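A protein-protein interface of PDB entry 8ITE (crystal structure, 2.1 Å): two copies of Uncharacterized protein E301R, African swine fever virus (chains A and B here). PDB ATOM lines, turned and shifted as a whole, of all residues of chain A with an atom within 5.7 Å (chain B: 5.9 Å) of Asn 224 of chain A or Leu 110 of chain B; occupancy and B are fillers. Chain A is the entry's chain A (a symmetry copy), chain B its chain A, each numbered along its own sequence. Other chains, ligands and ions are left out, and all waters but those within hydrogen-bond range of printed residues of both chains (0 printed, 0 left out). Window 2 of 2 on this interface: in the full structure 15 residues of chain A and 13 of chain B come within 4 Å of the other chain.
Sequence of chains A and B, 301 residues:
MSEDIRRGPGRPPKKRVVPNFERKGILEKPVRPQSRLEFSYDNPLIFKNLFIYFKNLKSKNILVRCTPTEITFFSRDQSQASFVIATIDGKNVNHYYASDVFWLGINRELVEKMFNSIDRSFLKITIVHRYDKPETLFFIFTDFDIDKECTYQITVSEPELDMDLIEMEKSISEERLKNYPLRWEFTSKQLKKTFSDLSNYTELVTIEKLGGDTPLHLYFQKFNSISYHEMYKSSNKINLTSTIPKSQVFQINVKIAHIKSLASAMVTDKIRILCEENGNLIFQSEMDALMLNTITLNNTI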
ATOM      1  N   LYS A 222      20.254  19.620 -20.216  1.00  0.00           N
ATOM      2  CA  LYS A 222      20.885  18.704 -19.287  1.00  0.00           C
ATOM      3  C   LYS A 222      20.402  17.310 -19.577  1.00  0.00           C
ATOM      4  O   LYS A 222      19.808  17.073 -20.622  1.00  0.00           O
ATOM      5  CB  LYS A 222      20.567  19.076 -17.843  1.00  0.00           C
ATOM      6  CG  LYS A 222      21.600  19.994 -17.222  1.00  0.00           C
ATOM      7  CD  LYS A 222      21.712  19.810 -15.722  1.00  0.00           C
ATOM      8  CE  LYS A 222      22.985  20.452 -15.200  1.00  0.00           C
ATOM      9  NZ  LYS A 222      23.099  20.388 -13.720  1.00  0.00           N
ATOM     10  N   PHE A 223      20.653  16.388 -18.659  1.00  0.00           N
ATOM     11  CA  PHE A 223      20.242  14.998 -18.848  1.00  0.00           C
ATOM     12  C   PHE A 223      18.892  14.763 -19.480  1.00  0.00           C
ATOM     13  O   PHE A 223      17.934  15.423 -19.127  1.00  0.00           O
ATOM     14  CB  PHE A 223      20.281  14.262 -17.506  1.00  0.00           C
ATOM     15  CG  PHE A 223      19.819  15.079 -16.325  1.00  0.00           C
ATOM     16  CD1 PHE A 223      18.495  15.094 -15.954  1.00  0.00           C
ATOM     17  CD2 PHE A 223      20.719  15.781 -15.550  1.00  0.00           C
ATOM     18  CE1 PHE A 223      18.073  15.828 -14.866  1.00  0.00           C
ATOM     19  CE2 PHE A 223      20.310  16.514 -14.461  1.00  0.00           C
ATOM     20  CZ  PHE A 223      18.982  16.539 -14.117  1.00  0.00           C
ATOM     21  N   ASN A 224      18.813  13.831 -20.412  1.00  0.00           N
ATOM     22  CA  ASN A 224      17.537  13.472 -21.033  1.00  0.00           C
ATOM     23  C   ASN A 224      16.738  14.592 -21.665  1.00  0.00           C
ATOM     24  O   ASN A 224      15.527  14.636 -21.476  1.00  0.00           O
ATOM     25  CB  ASN A 224      16.659  12.666 -20.072  1.00  0.00           C
ATOM     26  CG  ASN A 224      17.377  11.475 -19.484  1.00  0.00           C
ATOM     27  OD1 ASN A 224      17.667  10.506 -20.182  1.00  0.00           O
ATOM     28  ND2 ASN A 224      17.668  11.537 -18.192  1.00  0.00           N
ATOM     29  N   SER A 225      17.396  15.503 -22.367  1.00  0.00           N
ATOM     30  CA  SER A 225      16.720  16.567 -23.122  1.00  0.00           C
ATOM     31  C   SER A 225      15.865  17.472 -22.229  1.00  0.00           C
ATOM     32  O   SER A 225      14.817  17.972 -22.642  1.00  0.00           O
ATOM     33  CB  SER A 225      15.870  15.991 -24.261  1.00  0.00           C
ATOM     34  OG  SER A 225      16.672  15.607 -25.361  1.00  0.00           O
ATOM     35  N   ILE A 226      16.314  17.711 -21.002  1.00  0.00           N
ATOM     36  CA  ILE A 226      15.651  18.665 -20.117  1.00  0.00           C
ATOM     37  C   ILE A 226      16.295  20.035 -20.309  1.00  0.00           C
ATOM     38  O   ILE A 226      17.514  20.185 -20.160  1.00  0.00           O
ATOM     39  CB  ILE A 226      15.722  18.219 -18.650  1.00  0.00           C
ATOM     40  CG1 ILE A 226      14.897  16.948 -18.457  1.00  0.00           C
ATOM     41  CG2 ILE A 226      15.233  19.320 -17.741  1.00  0.00           C
ATOM     42  CD1 ILE A 226      15.259  16.179 -17.208  1.00  0.00           C
ATOM     43  N   ILE B 106       4.096  12.608 -14.338  1.00  0.00           N
ATOM     44  CA  ILE B 106       5.542  12.815 -14.356  1.00  0.00           C
ATOM     45  C   ILE B 106       6.248  11.460 -14.459  1.00  0.00           C
ATOM     46  O   ILE B 106       6.139  10.622 -13.551  1.00  0.00           O
ATOM     47  CB  ILE B 106       6.047  13.545 -13.104  1.00  0.00           C
ATOM     48  CG1 ILE B 106       5.321  14.860 -12.858  1.00  0.00           C
ATOM     49  CG2 ILE B 106       7.539  13.823 -13.240  1.00  0.00           C
ATOM     50  CD1 ILE B 106       5.740  15.463 -11.526  1.00  0.00           C
ATOM     51  N   ASN B 107       7.010  11.266 -15.534  1.00  0.00           N
ATOM     52  CA  ASN B 107       7.847  10.075 -15.644  1.00  0.00           C
ATOM     53  C   ASN B 107       8.966  10.146 -14.605  1.00  0.00           C
ATOM     54  O   ASN B 107       9.703  11.132 -14.554  1.00  0.00           O
ATOM     55  CB  ASN B 107       8.440   9.969 -17.049  1.00  0.00           C
ATOM     56  CG  ASN B 107       9.281   8.725 -17.227  1.00  0.00           C
ATOM     57  OD1 ASN B 107      10.446   8.691 -16.851  1.00  0.00           O
ATOM     58  ND2 ASN B 107       8.683   7.685 -17.780  1.00  0.00           N
ATOM     59  N   ARG B 108       9.097   9.100 -13.776  1.00  0.00           N
ATOM     60  CA  ARG B 108       9.982   9.190 -12.613  1.00  0.00           C
ATOM     61  C   ARG B 108      11.452   9.232 -13.026  1.00  0.00           C
ATOM     62  O   ARG B 108      12.223  10.063 -12.523  1.00  0.00           O
ATOM     63  CB  ARG B 108       9.725   8.021 -11.654  1.00  0.00           C
ATOM     64  CG  ARG B 108      10.425   8.197 -10.303  1.00  0.00           C
ATOM     65  CD  ARG B 108      10.808   6.883  -9.601  1.00  0.00           C
ATOM     66  NE  ARG B 108      11.468   5.925 -10.476  1.00  0.00           N
ATOM     67  CZ  ARG B 108      12.759   5.927 -10.784  1.00  0.00           C
ATOM     68  NH1 ARG B 108      13.575   6.849 -10.282  1.00  0.00           N
ATOM     69  NH2 ARG B 108      13.234   4.994 -11.601  1.00  0.00           N
ATOM     70  N   GLU B 109      11.871   8.339 -13.932  1.00  0.00           N
ATOM     71  CA  GLU B 109      13.272   8.347 -14.361  1.00  0.00           C
ATOM     72  C   GLU B 109      13.682   9.709 -14.923  1.00  0.00           C
ATOM     73  O   GLU B 109      14.823  10.140 -14.725  1.00  0.00           O
ATOM     74  CB  GLU B 109      13.506   7.229 -15.385  1.00  0.00           C
ATOM     75  CG  GLU B 109      14.964   6.882 -15.651  1.00  0.00           C
ATOM     76  CD  GLU B 109      15.120   5.645 -16.542  1.00  0.00           C
ATOM     77  OE1 GLU B 109      14.131   5.222 -17.184  1.00  0.00           O
ATOM     78  OE2 GLU B 109      16.236   5.089 -16.593  1.00  0.00           O
ATOM     79  N   LEU B 110      12.757  10.414 -15.588  1.00  0.00           N
ATOM     80  CA  LEU B 110      13.074  11.720 -16.170  1.00  0.00           C
ATOM     81  C   LEU B 110      13.499  12.742 -15.112  1.00  0.00           C
ATOM     82  O   LEU B 110      14.427  13.524 -15.341  1.00  0.00           O
ATOM     83  CB  LEU B 110      11.869  12.243 -16.950  1.00  0.00           C
ATOM     84  CG  LEU B 110      11.946  13.624 -17.602  1.00  0.00           C
ATOM     85  CD1 LEU B 110      13.068  13.674 -18.660  1.00  0.00           C
ATOM     86  CD2 LEU B 110      10.594  14.010 -18.207  1.00  0.00           C
ATOM     87  N   VAL B 111      12.858  12.745 -13.950  1.00  0.00           N
ATOM     88  CA  VAL B 111      13.166  13.708 -12.890  1.00  0.00           C
ATOM     89  C   VAL B 111      14.081  13.196 -11.815  1.00  0.00           C
ATOM     90  O   VAL B 111      14.405  13.916 -10.894  1.00  0.00           O
ATOM     91  CB  VAL B 111      11.895  14.146 -12.161  1.00  0.00           C
ATOM     92  CG1 VAL B 111      11.110  15.115 -12.992  1.00  0.00           C
ATOM     93  CG2 VAL B 111      11.035  12.967 -11.766  1.00  0.00           C
ATOM     94  N   GLU B 112      14.509  11.960 -11.926  1.00  0.00           N
ATOM     95  CA  GLU B 112      15.315  11.347 -10.882  1.00  0.00           C
ATOM     96  C   GLU B 112      16.630  12.032 -10.575  1.00  0.00           C
ATOM     97  O   GLU B 112      16.971  12.215  -9.429  1.00  0.00           O
ATOM     98  CB  GLU B 112      15.477   9.858 -11.200  1.00  0.00           C
ATOM     99  CG  GLU B 112      16.858   9.241 -11.180  1.00  0.00           C
ATOM    100  CD  GLU B 112      16.870   7.899 -11.876  1.00  0.00           C
ATOM    101  OE1 GLU B 112      17.353   7.829 -13.022  1.00  0.00           O
ATOM    102  OE2 GLU B 112      16.380   6.917 -11.288  1.00  0.00           O
ATOM    103  N   LYS B 113      17.327  12.465 -11.597  1.00  0.00           N
ATOM    104  CA  LYS B 113      18.583  13.129 -11.400  1.00  0.00           C
ATOM    105  C   LYS B 113      18.405  14.478 -10.763  1.00  0.00           C
ATOM    106  O   LYS B 113      19.129  14.830  -9.852  1.00  0.00           O
ATOM    107  CB  LYS B 113      19.280  13.267 -12.734  1.00  0.00           C
ATOM    108  CG  LYS B 113      20.033  12.019 -13.158  1.00  0.00           C
ATOM    109  CD  LYS B 113      19.630  11.579 -14.554  1.00  0.00           C
ATOM    110  CE  LYS B 113      20.836  11.122 -15.360  1.00  0.00           C
ATOM    111  NZ  LYS B 113      21.321   9.784 -14.927  1.00  0.00           N
ATOM    112  N   MET B 114      17.440  15.235 -11.246  1.00  0.00           N
ATOM    113  CA  MET B 114      17.168  16.526 -10.676  1.00  0.00           C
ATOM    114  C   MET B 114      16.876  16.416  -9.188  1.00  0.00           C
ATOM    115  O   MET B 114      17.473  17.096  -8.386  1.00  0.00           O
ATOM    116  CB  MET B 114      16.006  17.176 -11.412  1.00  0.00           C
ATOM    117  CG  MET B 114      15.516  18.469 -10.794  1.00  0.00           C
ATOM    118  SD  MET B 114      13.950  19.013 -11.474  1.00  0.00           S
ATOM    119  CE  MET B 114      12.862  17.800 -10.771  1.00  0.00           C
ATOM    120  N   ILE B 154      10.474  20.434 -16.898  1.00  0.00           N
ATOM    121  CA  ILE B 154      10.165  19.008 -16.914  1.00  0.00           C
ATOM    122  C   ILE B 154       8.899  18.809 -17.727  1.00  0.00           C
ATOM    123  O   ILE B 154       7.838  19.336 -17.372  1.00  0.00           O
ATOM    124  CB  ILE B 154       9.997  18.448 -15.493  1.00  0.00           C
ATOM    125  CG1 ILE B 154      11.305  18.587 -14.717  1.00  0.00           C
ATOM    126  CG2 ILE B 154       9.556  16.997 -15.548  1.00  0.00           C
ATOM    127  CD1 ILE B 154      12.467  17.824 -15.351  1.00  0.00           C
ATOM    128  N   THR B 155       8.996  18.057 -18.823  1.00  0.00           N
ATOM    129  CA  THR B 155       7.805  17.827 -19.630  1.00  0.00           C
ATOM    130  C   THR B 155       6.886  16.869 -18.890  1.00  0.00           C
ATOM    131  O   THR B 155       7.340  15.876 -18.314  1.00  0.00           O
ATOM    132  CB  THR B 155       8.164  17.269 -21.010  1.00  0.00           C
ATOM    133  OG1 THR B 155       8.603  15.919 -20.870  1.00  0.00           O
ATOM    134  CG2 THR B 155       9.271  18.100 -21.655  1.00  0.00           C
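CB of Lys 113 of chain B touches CE1 of Phe 223 of chain A, 3.5 Å away.
Phe 223 of chain A touches Met 114 of chain B.
O of Asn 224 of chain A touches CD1 of Leu 110 of chain B (3.9 Å).
CD1 of Ile 226 of chain A touches O of Leu 110 of chain B, at 3.4 Å.
CD1 of Ile 226 of chain A touches CD1 of Ile 154 of chain B, 3.7 Å away.
No position is printed for both chains.
The backbone NH (N) of Leu 110 of chain B sits at hydrogen-bond distance from the side-chain amide oxygen (OD1) of Asn 107 of chain B (3.1 Å).
Hydrophobic or aromatic side chains of chain A that line the printed part of chain B: Phe 223 and Ile 226.
Of the 11 printed residues of chain B, 4 touch a printed residue of chain A.
Among the printed residues, 5 pairs touch across the chains.
Among the printed residues, no Asp or Glu carboxylate lies within 4 Å of a Lys or Arg side-chain nitrogen of the other chain.
Of chain B, only Leu 110 comes within 4 Å of Asn 224 of chain A.
Of chain A, only Asn 224 and Ile 226 come within 4 Å of Leu 110 of chain B.
Printed residues of chain B within 4 Å of Ile 226 of chain A: Leu 110 and Ile 154.
Of the printed residues of chain B, Phe 223 of chain A touches Lys 113 and Met 114.
Printed residues of chain A within 4 Å of Met 114 of chain B: Phe 223 (3.5 Å).
Glu 109 of chain B touches none of the printed residues of chain A.
The nearest residue of chain B that does not touch Asn 224 of chain A is Lys 113 of chain B (4.1 Å).
The nearest residue of chain A that does not touch Leu 110 of chain B is Phe 223 of chain A (4.3 Å).
The nearest printed residue of chain A that does not touch Ile 154 of chain B is Phe 223 of chain A (6.0 Å).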
